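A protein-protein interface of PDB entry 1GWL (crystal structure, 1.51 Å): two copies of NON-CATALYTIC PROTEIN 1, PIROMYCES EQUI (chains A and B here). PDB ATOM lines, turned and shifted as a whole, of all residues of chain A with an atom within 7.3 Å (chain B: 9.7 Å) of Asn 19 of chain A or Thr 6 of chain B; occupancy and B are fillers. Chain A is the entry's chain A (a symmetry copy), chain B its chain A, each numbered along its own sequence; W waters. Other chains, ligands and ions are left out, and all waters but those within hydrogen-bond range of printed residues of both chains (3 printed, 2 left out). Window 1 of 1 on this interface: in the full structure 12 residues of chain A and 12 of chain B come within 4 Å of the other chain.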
ATOM      1  N   THR A   8       3.132   7.839   1.730  1.00  0.00           N
ATOM      2  CA  THR A   8       4.604   7.789   1.817  1.00  0.00           C
ATOM      3  C   THR A   8       5.013   6.426   2.371  1.00  0.00           C
ATOM      4  O   THR A   8       4.760   6.114   3.531  1.00  0.00           O
ATOM      5  CB  THR A   8       5.140   8.903   2.720  1.00  0.00           C
ATOM      6  OG1 THR A   8       4.777  10.201   2.220  1.00  0.00           O
ATOM      7  CG2 THR A   8       6.682   8.946   2.768  1.00  0.00           C
ATOM      8  N   VAL A   9       5.675   5.633   1.548  1.00  0.00           N
ATOM      9  CA  VAL A   9       6.170   4.316   1.954  1.00  0.00           C
ATOM     10  C   VAL A   9       7.509   4.535   2.669  1.00  0.00           C
ATOM     11  O   VAL A   9       8.466   4.942   2.031  1.00  0.00           O
ATOM     12  CB  VAL A   9       6.322   3.338   0.751  1.00  0.00           C
ATOM     13  CG1 VAL A   9       6.808   1.993   1.243  1.00  0.00           C
ATOM     14  CG2 VAL A   9       4.995   3.193   0.007  1.00  0.00           C
ATOM     15  N   ILE A  10       7.554   4.256   3.969  1.00  0.00           N
ATOM     16  CA  ILE A  10       8.780   4.427   4.774  1.00  0.00           C
ATOM     17  C   ILE A  10       9.631   3.173   4.692  1.00  0.00           C
ATOM     18  O   ILE A  10      10.823   3.246   4.355  1.00  0.00           O
ATOM     19  CB  ILE A  10       8.467   4.894   6.198  1.00  0.00           C
ATOM     20  CG1 ILE A  10       7.718   6.251   6.152  1.00  0.00           C
ATOM     21  CG2 ILE A  10       9.741   5.049   7.006  1.00  0.00           C
ATOM     22  CD1 ILE A  10       7.227   6.701   7.493  1.00  0.00           C
ATOM     23  N   PHE A  11       9.027   2.009   4.911  1.00  0.00           N
ATOM     24  CA  PHE A  11       9.674   0.796   4.424  1.00  0.00           C
ATOM     25  C   PHE A  11       8.719  -0.349   4.204  1.00  0.00           C
ATOM     26  O   PHE A  11       7.714  -0.484   4.895  1.00  0.00           O
ATOM     27  CB  PHE A  11      10.801   0.349   5.321  1.00  0.00           C
ATOM     28  CG  PHE A  11      10.388   0.097   6.748  1.00  0.00           C
ATOM     29  CD1 PHE A  11      10.541   1.071   7.677  1.00  0.00           C
ATOM     30  CD2 PHE A  11       9.991  -1.176   7.155  1.00  0.00           C
ATOM     31  CE1 PHE A  11      10.214   0.837   9.011  1.00  0.00           C
ATOM     32  CE2 PHE A  11       9.618  -1.404   8.461  1.00  0.00           C
ATOM     33  CZ  PHE A  11       9.761  -0.404   9.389  1.00  0.00           C
ATOM     34  N   GLY A  16      17.658  -2.804   6.442  1.00  0.00           N
ATOM     35  CA  GLY A  16      18.470  -1.689   6.938  1.00  0.00           C
ATOM     36  C   GLY A  16      17.554  -0.485   7.115  1.00  0.00           C
ATOM     37  O   GLY A  16      16.333  -0.571   6.934  1.00  0.00           O
ATOM     38  N   LEU A  17      18.128   0.665   7.470  1.00  0.00           N
ATOM     39  CA  LEU A  17      17.270   1.841   7.688  1.00  0.00           C
ATOM     40  C   LEU A  17      16.723   2.396   6.376  1.00  0.00           C
ATOM     41  O   LEU A  17      17.409   2.315   5.365  1.00  0.00           O
ATOM     42  CB  LEU A  17      18.063   2.943   8.409  1.00  0.00           C
ATOM     43  CG  LEU A  17      18.447   2.674   9.868  1.00  0.00           C
ATOM     44  CD1 LEU A  17      19.491   3.702  10.347  1.00  0.00           C
ATOM     45  CD2 LEU A  17      17.296   2.624  10.773  1.00  0.00           C
ATOM     46  N   PRO A  18      15.538   3.004   6.406  1.00  0.00           N
ATOM     47  CA  PRO A  18      14.979   3.691   5.226  1.00  0.00           C
ATOM     48  C   PRO A  18      15.886   4.816   4.734  1.00  0.00           C
ATOM     49  O   PRO A  18      16.499   5.493   5.544  1.00  0.00           O
ATOM     50  CB  PRO A  18      13.689   4.298   5.755  1.00  0.00           C
ATOM     51  CG  PRO A  18      13.410   3.686   7.004  1.00  0.00           C
ATOM     52  CD  PRO A  18      14.646   3.073   7.571  1.00  0.00           C
ATOM     53  N   ASN A  19      15.934   5.044   3.424  1.00  0.00           N
ATOM     54  CA  ASN A  19      16.694   6.149   2.849  1.00  0.00           C
ATOM     55  C   ASN A  19      16.152   7.459   3.454  1.00  0.00           C
ATOM     56  O   ASN A  19      14.943   7.670   3.522  1.00  0.00           O
ATOM     57  CB  ASN A  19      16.583   6.165   1.316  1.00  0.00           C
ATOM     58  CG  ASN A  19      17.399   7.264   0.677  1.00  0.00           C
ATOM     59  OD1 ASN A  19      18.610   7.370   0.898  1.00  0.00           O
ATOM     60  ND2 ASN A  19      16.738   8.101  -0.136  1.00  0.00           N
ATOM     61  N   GLY A  20      17.071   8.335   3.851  1.00  0.00           N
ATOM     62  CA  GLY A  20      16.752   9.625   4.454  1.00  0.00           C
ATOM     63  C   GLY A  20      16.263   9.616   5.887  1.00  0.00           C
ATOM     64  O   GLY A  20      15.724  10.648   6.338  1.00  0.00           O
ATOM     65  N   TYR A  21      16.452   8.501   6.602  1.00  0.00           N
ATOM     66  CA  TYR A  21      16.159   8.397   8.027  1.00  0.00           C
ATOM     67  C   TYR A  21      17.401   7.967   8.814  1.00  0.00           C
ATOM     68  O   TYR A  21      18.232   7.178   8.332  1.00  0.00           O
ATOM     69  CB  TYR A  21      15.041   7.398   8.262  1.00  0.00           C
ATOM     70  CG  TYR A  21      13.675   7.906   7.821  1.00  0.00           C
ATOM     71  CD1 TYR A  21      13.335   8.014   6.475  1.00  0.00           C
ATOM     72  CD2 TYR A  21      12.737   8.258   8.732  1.00  0.00           C
ATOM     73  CE1 TYR A  21      12.092   8.487   6.075  1.00  0.00           C
ATOM     74  CE2 TYR A  21      11.478   8.721   8.347  1.00  0.00           C
ATOM     75  CZ  TYR A  21      11.162   8.847   7.033  1.00  0.00           C
ATOM     76  OH  TYR A  21       9.929   9.350   6.628  1.00  0.00           O
ATOM     77  N   ASP A  22      17.516   8.523  10.016  1.00  0.00           N
ATOM     78  CA  ASP A  22      18.484   8.093  11.028  1.00  0.00           C
ATOM     79  C   ASP A  22      17.734   7.371  12.167  1.00  0.00           C
ATOM     80  O   ASP A  22      16.518   7.480  12.276  1.00  0.00           O
ATOM     81  CB  ASP A  22      19.215   9.304  11.586  1.00  0.00           C
ATOM     82  CG  ASP A  22      20.315   9.817  10.680  1.00  0.00           C
ATOM     83  OD1 ASP A  22      20.422   9.411   9.499  1.00  0.00           O
ATOM     84  OD2 ASP A  22      21.145  10.650  11.087  1.00  0.00           O
ATOM     85  N   ARG A  53      13.296  11.474  10.427  1.00  0.00           N
ATOM     86  CA  ARG A  53      13.314  11.993   9.071  1.00  0.00           C
ATOM     87  C   ARG A  53      14.326  13.125   8.981  1.00  0.00           C
ATOM     88  O   ARG A  53      14.191  14.142   9.671  1.00  0.00           O
ATOM     89  CB  ARG A  53      11.895  12.469   8.701  1.00  0.00           C
ATOM     90  CG  ARG A  53      11.718  12.818   7.293  1.00  0.00           C
ATOM     91  CD  ARG A  53      10.253  13.176   6.983  1.00  0.00           C
ATOM     92  NE  ARG A  53      10.178  13.908   5.751  1.00  0.00           N
ATOM     93  CZ  ARG A  53       9.059  14.176   5.113  1.00  0.00           C
ATOM     94  NH1 ARG A  53       7.919  13.714   5.567  1.00  0.00           N
ATOM     95  NH2 ARG A  53       9.096  14.872   3.980  1.00  0.00           N
ATOM     96  N   ASN A  54      15.349  12.970   8.155  1.00  0.00           N
ATOM     97  CA  ASN A  54      16.418  13.964   8.090  1.00  0.00           C
ATOM     98  C   ASN A  54      15.989  15.292   7.482  1.00  0.00           C
ATOM     99  O   ASN A  54      16.450  16.344   7.938  1.00  0.00           O
ATOM    100  CB  ASN A  54      17.630  13.413   7.335  1.00  0.00           C
ATOM    101  CG  ASN A  54      18.293  12.218   8.038  1.00  0.00           C
ATOM    102  OD1 ASN A  54      18.892  11.363   7.374  1.00  0.00           O
ATOM    103  ND2 ASN A  54      18.199  12.153   9.367  1.00  0.00           N
ATOM    104  N   ASN B   2      24.724   3.326   1.445  1.00  0.00           N
ATOM    105  CA  ASN B   2      23.459   2.650   1.031  1.00  0.00           C
ATOM    106  C   ASN B   2      22.966   2.897  -0.389  1.00  0.00           C
ATOM    107  O   ASN B   2      23.261   3.901  -1.035  1.00  0.00           O
ATOM    108  CB  ASN B   2      22.310   2.952   2.012  1.00  0.00           C
ATOM    109  CG  ASN B   2      22.093   4.445   2.244  1.00  0.00           C
ATOM    110  OD1 ASN B   2      21.537   5.150   1.385  1.00  0.00           O
ATOM    111  ND2 ASN B   2      22.486   4.925   3.428  1.00  0.00           N
ATOM    112  N   VAL B   3      22.158   1.947  -0.844  1.00  0.00           N
ATOM    113  CA  VAL B   3      21.686   1.843  -2.220  1.00  0.00           C
ATOM    114  C   VAL B   3      20.182   2.171  -2.253  1.00  0.00           C
ATOM    115  O   VAL B   3      19.567   2.317  -3.332  1.00  0.00           O
ATOM    116  CB  VAL B   3      21.961   0.387  -2.711  1.00  0.00           C
ATOM    117  CG1 VAL B   3      21.364   0.097  -4.105  1.00  0.00           C
ATOM    118  CG2 VAL B   3      23.452   0.126  -2.725  1.00  0.00           C
ATOM    119  N   ARG B   4      19.589   2.209  -1.063  1.00  0.00           N
ATOM    120  CA  ARG B   4      18.151   2.345  -0.907  1.00  0.00           C
ATOM    121  C   ARG B   4      17.676   3.717  -1.361  1.00  0.00           C
ATOM    122  O   ARG B   4      18.286   4.728  -1.086  1.00  0.00           O
ATOM    123  CB  ARG B   4      17.683   2.094   0.546  1.00  0.00           C
ATOM    124  CG  ARG B   4      16.163   2.055   0.705  1.00  0.00           C
ATOM    125  CD  ARG B   4      15.675   1.428   2.017  1.00  0.00           C
ATOM    126  NE  ARG B   4      15.849  -0.013   1.995  1.00  0.00           N
ATOM    127  CZ  ARG B   4      16.764  -0.700   2.677  1.00  0.00           C
ATOM    128  NH1 ARG B   4      17.622  -0.120   3.531  1.00  0.00           N
ATOM    129  NH2 ARG B   4      16.808  -2.021   2.513  1.00  0.00           N
ATOM    130  N   ALA B   5      16.589   3.694  -2.079  1.00  0.00           N
ATOM    131  CA  ALA B   5      15.947   4.895  -2.595  1.00  0.00           C
ATOM    132  C   ALA B   5      14.684   5.177  -1.818  1.00  0.00           C
ATOM    133  O   ALA B   5      14.211   4.356  -1.054  1.00  0.00           O
ATOM    134  CB  ALA B   5      15.608   4.685  -4.022  1.00  0.00           C
ATOM    135  N   THR B   6      14.198   6.393  -1.999  1.00  0.00           N
ATOM    136  CA  THR B   6      12.864   6.824  -1.587  1.00  0.00           C
ATOM    137  C   THR B   6      11.955   6.810  -2.835  1.00  0.00           C
ATOM    138  O   THR B   6      12.263   7.516  -3.859  1.00  0.00           O
ATOM    139  CB  THR B   6      12.947   8.254  -0.984  1.00  0.00           C
ATOM    140  OG1 THR B   6      13.748   8.248   0.208  1.00  0.00           O
ATOM    141  CG2 THR B   6      11.515   8.800  -0.566  1.00  0.00           C
ATOM    142  N   TYR B   7      10.876   6.025  -2.784  1.00  0.00           N
ATOM    143  CA  TYR B   7       9.898   5.866  -3.881  1.00  0.00           C
ATOM    144  C   TYR B   7       8.612   6.655  -3.589  1.00  0.00           C
ATOM    145  O   TYR B   7       7.913   6.332  -2.596  1.00  0.00           O
ATOM    146  CB  TYR B   7       9.515   4.404  -4.076  1.00  0.00           C
ATOM    147  CG  TYR B   7      10.642   3.532  -4.527  1.00  0.00           C
ATOM    148  CD1 TYR B   7      11.502   2.987  -3.620  1.00  0.00           C
ATOM    149  CD2 TYR B   7      10.902   3.339  -5.883  1.00  0.00           C
ATOM    150  CE1 TYR B   7      12.581   2.213  -4.011  1.00  0.00           C
ATOM    151  CE2 TYR B   7      11.968   2.568  -6.298  1.00  0.00           C
ATOM    152  CZ  TYR B   7      12.811   2.004  -5.364  1.00  0.00           C
ATOM    153  OH  TYR B   7      13.882   1.215  -5.728  1.00  0.00           O
ATOM    154  N   THR B   8       8.297   7.622  -4.447  1.00  0.00           N
ATOM    155  CA  THR B   8       7.108   8.486  -4.327  1.00  0.00           C
ATOM    156  C   THR B   8       6.067   8.027  -5.346  1.00  0.00           C
ATOM    157  O   THR B   8       6.259   8.164  -6.550  1.00  0.00           O
ATOM    158  CB  THR B   8       7.467   9.954  -4.572  1.00  0.00           C
ATOM    159  OG1 THR B   8       8.442  10.418  -3.623  1.00  0.00           O
ATOM    160  CG2 THR B   8       6.271  10.907  -4.367  1.00  0.00           C
ATOM    161  N   VAL B   9       4.952   7.515  -4.855  1.00  0.00           N
ATOM    162  CA  VAL B   9       3.847   7.074  -5.709  1.00  0.00           C
ATOM    163  C   VAL B   9       3.014   8.316  -6.051  1.00  0.00           C
ATOM    164  O   VAL B   9       2.395   8.882  -5.166  1.00  0.00           O
ATOM    165  CB  VAL B   9       2.974   5.974  -5.036  1.00  0.00           C
ATOM    166  CG1 VAL B   9       1.873   5.545  -5.979  1.00  0.00           C
ATOM    167  CG2 VAL B   9       3.836   4.777  -4.633  1.00  0.00           C
ATOM    168  N   ARG B  53       3.622  19.809  -9.113  1.00  0.00           N
ATOM    169  CA  ARG B  53       3.709  19.594  -7.680  1.00  0.00           C
ATOM    170  C   ARG B  53       3.552  20.925  -6.962  1.00  0.00           C
ATOM    171  O   ARG B  53       4.358  21.842  -7.159  1.00  0.00           O
ATOM    172  CB  ARG B  53       5.064  18.931  -7.358  1.00  0.00           C
ATOM    173  CG  ARG B  53       5.199  18.462  -5.980  1.00  0.00           C
ATOM    174  CD  ARG B  53       6.530  17.716  -5.768  1.00  0.00           C
ATOM    175  NE  ARG B  53       6.834  17.647  -4.368  1.00  0.00           N
ATOM    176  CZ  ARG B  53       7.788  16.901  -3.851  1.00  0.00           C
ATOM    177  NH1 ARG B  53       8.493  16.111  -4.625  1.00  0.00           N
ATOM    178  NH2 ARG B  53       7.997  16.915  -2.538  1.00  0.00           N
ATOM    179  N   PHE B  58      11.350  17.427  -6.830  1.00  0.00           N
ATOM    180  CA  PHE B  58      12.151  16.215  -6.985  1.00  0.00           C
ATOM    181  C   PHE B  58      13.546  16.604  -7.439  1.00  0.00           C
ATOM    182  O   PHE B  58      13.730  17.653  -8.078  1.00  0.00           O
ATOM    183  CB  PHE B  58      11.527  15.284  -8.037  1.00  0.00           C
ATOM    184  CG  PHE B  58      10.179  14.725  -7.652  1.00  0.00           C
ATOM    185  CD1 PHE B  58      10.060  13.785  -6.636  1.00  0.00           C
ATOM    186  CD2 PHE B  58       9.034  15.162  -8.314  1.00  0.00           C
ATOM    187  CE1 PHE B  58       8.806  13.283  -6.281  1.00  0.00           C
ATOM    188  CE2 PHE B  58       7.791  14.676  -7.964  1.00  0.00           C
ATOM    189  CZ  PHE B  58       7.677  13.721  -6.942  1.00  0.00           C
ATOM    190  N   ARG B  59      14.536  15.773  -7.131  1.00  0.00           N
ATOM    191  CA  ARG B  59      15.904  15.970  -7.625  1.00  0.00           C
ATOM    192  C   ARG B  59      16.459  14.706  -8.291  1.00  0.00           C
ATOM    193  O   ARG B  59      16.523  13.638  -7.653  1.00  0.00           O
ATOM    194  CB  ARG B  59      16.825  16.426  -6.491  1.00  0.00           C
ATOM    195  CG  ARG B  59      16.524  17.804  -6.001  1.00  0.00           C
ATOM    196  CD  ARG B  59      17.425  18.191  -4.858  1.00  0.00           C
ATOM    197  NE  ARG B  59      16.948  17.694  -3.577  1.00  0.00           N
ATOM    198  CZ  ARG B  59      17.663  17.696  -2.449  1.00  0.00           C
ATOM    199  NH1 ARG B  59      18.925  18.142  -2.417  1.00  0.00           N
ATOM    200  NH2 ARG B  59      17.106  17.275  -1.317  1.00  0.00           N
ATOM    201  N   GLY B  60      16.844  14.783  -9.565  1.00  0.00           N
ATOM    202  CA  GLY B  60      17.418  13.653 -10.267  1.00  0.00           C
ATOM    203  C   GLY B  60      16.586  12.393 -10.167  1.00  0.00           C
ATOM    204  O   GLY B  60      15.352  12.436 -10.270  1.00  0.00           O
ATOM    205  N   GLY B  61      17.259  11.275  -9.944  1.00  0.00           N
ATOM    206  CA  GLY B  61      16.588   9.995  -9.851  1.00  0.00           C
ATOM    207  C   GLY B  61      16.024   9.481 -11.155  1.00  0.00           C
ATOM    208  O   GLY B  61      16.624   9.669 -12.233  1.00  0.00           O
ATOM    209  N   SER B  62      14.867   8.829 -11.071  1.00  0.00           N
ATOM    210  CA  SER B  62      14.267   8.148 -12.212  1.00  0.00           C
ATOM    211  C   SER B  62      12.736   8.182 -12.107  1.00  0.00           C
ATOM    212  O   SER B  62      12.166   8.302 -11.001  1.00  0.00           O
ATOM    213  CB  SER B  62      14.794   6.701 -12.344  1.00  0.00           C
ATOM    214  OG  SER B  62      14.728   5.966 -11.118  1.00  0.00           O
ATOM    215  N   LEU B  63      12.073   8.143 -13.260  1.00  0.00           N
ATOM    216  CA  LEU B  63      10.613   8.102 -13.392  1.00  0.00           C
ATOM    217  C   LEU B  63      10.197   6.767 -14.015  1.00  0.00           C
ATOM    218  O   LEU B  63      10.729   6.336 -15.053  1.00  0.00           O
ATOM    219  CB  LEU B  63      10.084   9.259 -14.264  1.00  0.00           C
ATOM    220  CG  LEU B  63      10.231  10.670 -13.672  1.00  0.00           C
ATOM    221  CD1 LEU B  63       9.985  11.734 -14.739  1.00  0.00           C
ATOM    222  CD2 LEU B  63       9.293  10.867 -12.483  1.00  0.00           C
ATOM    223  N   VAL B 131       5.566   6.589 -10.700  1.00  0.00           N
ATOM    224  CA  VAL B 131       6.380   6.600  -9.472  1.00  0.00           C
ATOM    225  C   VAL B 131       7.737   7.253  -9.709  1.00  0.00           C
ATOM    226  O   VAL B 131       8.378   6.999 -10.743  1.00  0.00           O
ATOM    227  CB  VAL B 131       6.651   5.162  -8.995  1.00  0.00           C
ATOM    228  CG1 VAL B 131       7.439   5.118  -7.660  1.00  0.00           C
ATOM    229  CG2 VAL B 131       5.352   4.340  -8.884  1.00  0.00           C
ATOM    230  N   HIS B 132       8.178   8.107  -8.785  1.00  0.00           N
ATOM    231  CA  HIS B 132       9.550   8.659  -8.800  1.00  0.00           C
ATOM    232  C   HIS B 132      10.427   7.926  -7.807  1.00  0.00           C
ATOM    233  O   HIS B 132       9.998   7.608  -6.706  1.00  0.00           O
ATOM    234  CB  HIS B 132       9.582  10.166  -8.483  1.00  0.00           C
ATOM    235  CG  HIS B 132      10.976  10.733  -8.405  1.00  0.00           C
ATOM    236  ND1 HIS B 132      11.648  10.896  -7.205  1.00  0.00           N
ATOM    237  CD2 HIS B 132      11.812  11.176  -9.378  1.00  0.00           C
ATOM    238  CE1 HIS B 132      12.842  11.409  -7.456  1.00  0.00           C
ATOM    239  NE2 HIS B 132      12.973  11.590  -8.762  1.00  0.00           N
ATOM    240  N   SER B 133      11.663   7.610  -8.190  1.00  0.00           N
ATOM    241  CA  SER B 133      12.701   7.140  -7.267  1.00  0.00           C
ATOM    242  C   SER B 133      13.850   8.153  -7.184  1.00  0.00           C
ATOM    243  O   SER B 133      14.260   8.711  -8.186  1.00  0.00           O
ATOM    244  CB  SER B 133      13.259   5.802  -7.741  1.00  0.00           C
ATOM    245  OG  SER B 133      14.397   5.437  -6.972  1.00  0.00           O
ATOM    246  N   THR B 134      14.406   8.355  -5.995  1.00  0.00           N
ATOM    247  CA  THR B 134      15.658   9.129  -5.827  1.00  0.00           C
ATOM    248  C   THR B 134      16.892   8.467  -6.418  1.00  0.00           C
ATOM    249  O   THR B 134      17.919   9.140  -6.642  1.00  0.00           O
ATOM    250  CB  THR B 134      15.929   9.444  -4.343  1.00  0.00           C
ATOM    251  OG1 THR B 134      15.988   8.217  -3.586  1.00  0.00           O
ATOM    252  CG2 THR B 134      14.778  10.272  -3.743  1.00  0.00           C
ATOM    253  N   GLY B 135      16.805   7.166  -6.689  1.00  0.00           N
ATOM    254  CA  GLY B 135      17.916   6.391  -7.252  1.00  0.00           C
ATOM    255  C   GLY B 135      17.837   6.230  -8.764  1.00  0.00           C
ATOM    256  O   GLY B 135      16.898   6.705  -9.398  1.00  0.00           O
ATOM    257  N   SER B 136      18.857   5.553  -9.338  1.00  0.00           N
ATOM    258  CA  SER B 136      18.946   5.354 -10.777  1.00  0.00           C
ATOM    259  C   SER B 136      17.931   4.336 -11.311  1.00  0.00           C
ATOM    260  O   SER B 136      17.417   3.479 -10.575  1.00  0.00           O
ATOM    261  CB  SER B 136      20.355   4.884 -11.184  1.00  0.00           C
ATOM    262  OG  SER B 136      20.546   3.546 -10.767  1.00  0.00           O
ATOM    263  N   ASP B 139      18.926   0.681 -10.763  1.00  0.00           N
ATOM    264  CA  ASP B 139      18.740   0.218  -9.377  1.00  0.00           C
ATOM    265  C   ASP B 139      17.269   0.198  -8.922  1.00  0.00           C
ATOM    266  O   ASP B 139      16.988  -0.155  -7.764  1.00  0.00           O
ATOM    267  CB  ASP B 139      19.545   1.101  -8.414  1.00  0.00           C
ATOM    268  CG  ASP B 139      21.058   0.976  -8.605  1.00  0.00           C
ATOM    269  OD1 ASP B 139      21.544  -0.060  -9.123  1.00  0.00           O
ATOM    270  OD2 ASP B 139      21.830   1.894  -8.225  1.00  0.00           O
ATOM    271  N   PHE B 140      16.335   0.577  -9.791  1.00  0.00           N
ATOM    272  CA  PHE B 140      14.914   0.712  -9.427  1.00  0.00           C
ATOM    273  C   PHE B 140      14.268  -0.658  -9.176  1.00  0.00           C
ATOM    274  O   PHE B 140      14.285  -1.525 -10.037  1.00  0.00           O
ATOM    275  CB  PHE B 140      14.193   1.453 -10.566  1.00  0.00           C
ATOM    276  CG  PHE B 140      12.789   1.958 -10.225  1.00  0.00           C
ATOM    277  CD1 PHE B 140      11.723   1.069 -10.124  1.00  0.00           C
ATOM    278  CD2 PHE B 140      12.528   3.311 -10.070  1.00  0.00           C
ATOM    279  CE1 PHE B 140      10.442   1.541  -9.875  1.00  0.00           C
ATOM    280  CE2 PHE B 140      11.211   3.768  -9.813  1.00  0.00           C
ATOM    281  CZ  PHE B 140      10.203   2.852  -9.702  1.00  0.00           C
ATOM    282  N   VAL B 141      13.748  -0.870  -7.971  1.00  0.00           N
ATOM    283  CA  VAL B 141      13.037  -2.104  -7.628  1.00  0.00           C
ATOM    284  C   VAL B 141      11.594  -1.720  -7.315  1.00  0.00           C
ATOM    285  O   VAL B 141      11.333  -1.001  -6.358  1.00  0.00           O
ATOM    286  CB  VAL B 141      13.699  -2.820  -6.436  1.00  0.00           C
ATOM    287  CG1 VAL B 141      12.921  -4.106  -6.031  1.00  0.00           C
ATOM    288  CG2 VAL B 141      15.149  -3.198  -6.746  1.00  0.00           C
HETATM  289  O   HOH W   1      12.741   6.706   2.223  1.00  0.00           O
HETATM  290  O   HOH W   2      19.576   4.194   4.344  1.00  0.00           O
HETATM  291  O   HOH W   3      10.237   4.594  -0.290  1.00  0.00           O
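Water W1 bridges OG1 of Thr 6 of chain B (2.7 Å) and O of Asn 19 of chain A (2.7 Å).
Water W3 lies within hydrogen-bond range of the backbone carbonyl oxygen (O) of Val 9 of chain A (2.9 Å) and the backbone NH (N) of Tyr 7 of chain B (2.9 Å).
Water W2 bridges the backbone carbonyl oxygen of Leu 17 of chain A (3.0 Å) and the side-chain amide nitrogen of Asn 2 of chain B (3.1 Å).
Positions printed for both chains: 8, 9 and 53.
Along chain A the printed residues that touch a printed residue of chain B span positions 16 to 19.
Of the 24 printed residues of chain B, 5 touch a printed residue of chain A.
Among the printed residues, 8 pairs touch across the chains.
N of Thr 6 of chain B sits at hydrogen-bond distance from OG1 of Thr 134 of chain B (3.0 Å).
Of the printed residues of chain B, Asn 19 of chain A touches Asn 2 (3.7 Å), Arg 4 (3.2 Å), Ala 5 (3.8 Å), Thr 6 (3.0 Å) and Thr 134 (3.5 Å).
Of the printed residues of chain A, Thr 6 of chain B touches Asn 19.
No residue of chain B comes within 4 Å of Gly 20 of chain A.
Printed residues of chain A within 4 Å of Arg 4 of chain B: Gly 16 (3.6 Å), Leu 17 (3.1 Å), Pro 18 (3.99 Å) and Asn 19 (3.2 Å).
Printed residues of chain A within 4 Å of Ala 5 of chain B: Asn 19 (3.8 Å).
Arg 53 of chain A touches none of the printed residues of chain B.
Val 141 of chain B touches none of the printed residues of chain A.
The nearest residue of chain A that does not touch Thr 6 of chain B is Gly 20 of chain A (4.9 Å).
The nearest printed residue of chain A that does not touch Ala 5 of chain B is Pro 18 of chain A (6.0 Å).
The guanidinium group of Arg 4 of chain B is in hydrogen-bond range of the backbone carbonyl oxygen of Leu 17 of chain A, at 3.1 Å.
ND2 of Asn 19 of chain A is in hydrogen-bond range of OG1 of Thr 6 of chain B, 3.0 Å away.
The backbone carbonyl oxygen of Arg 4 of chain B sits close to the side-chain amide oxygen of Asn 19 of chain A, 3.3 Å away.
Among the printed residues, merely in contact across the chains: Gly 16 of chain A with Arg 4 of chain B (3.6 Å), Pro 18 of chain A with Arg 4 of chain B (3.99 Å), Asn 19 of chain A with Asn 2 of chain B (3.7 Å), Asn 19 of chain A with Ala 5 of chain B (3.8 Å) and Asn 19 of chain A with Thr 134 of chain B (3.5 Å).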
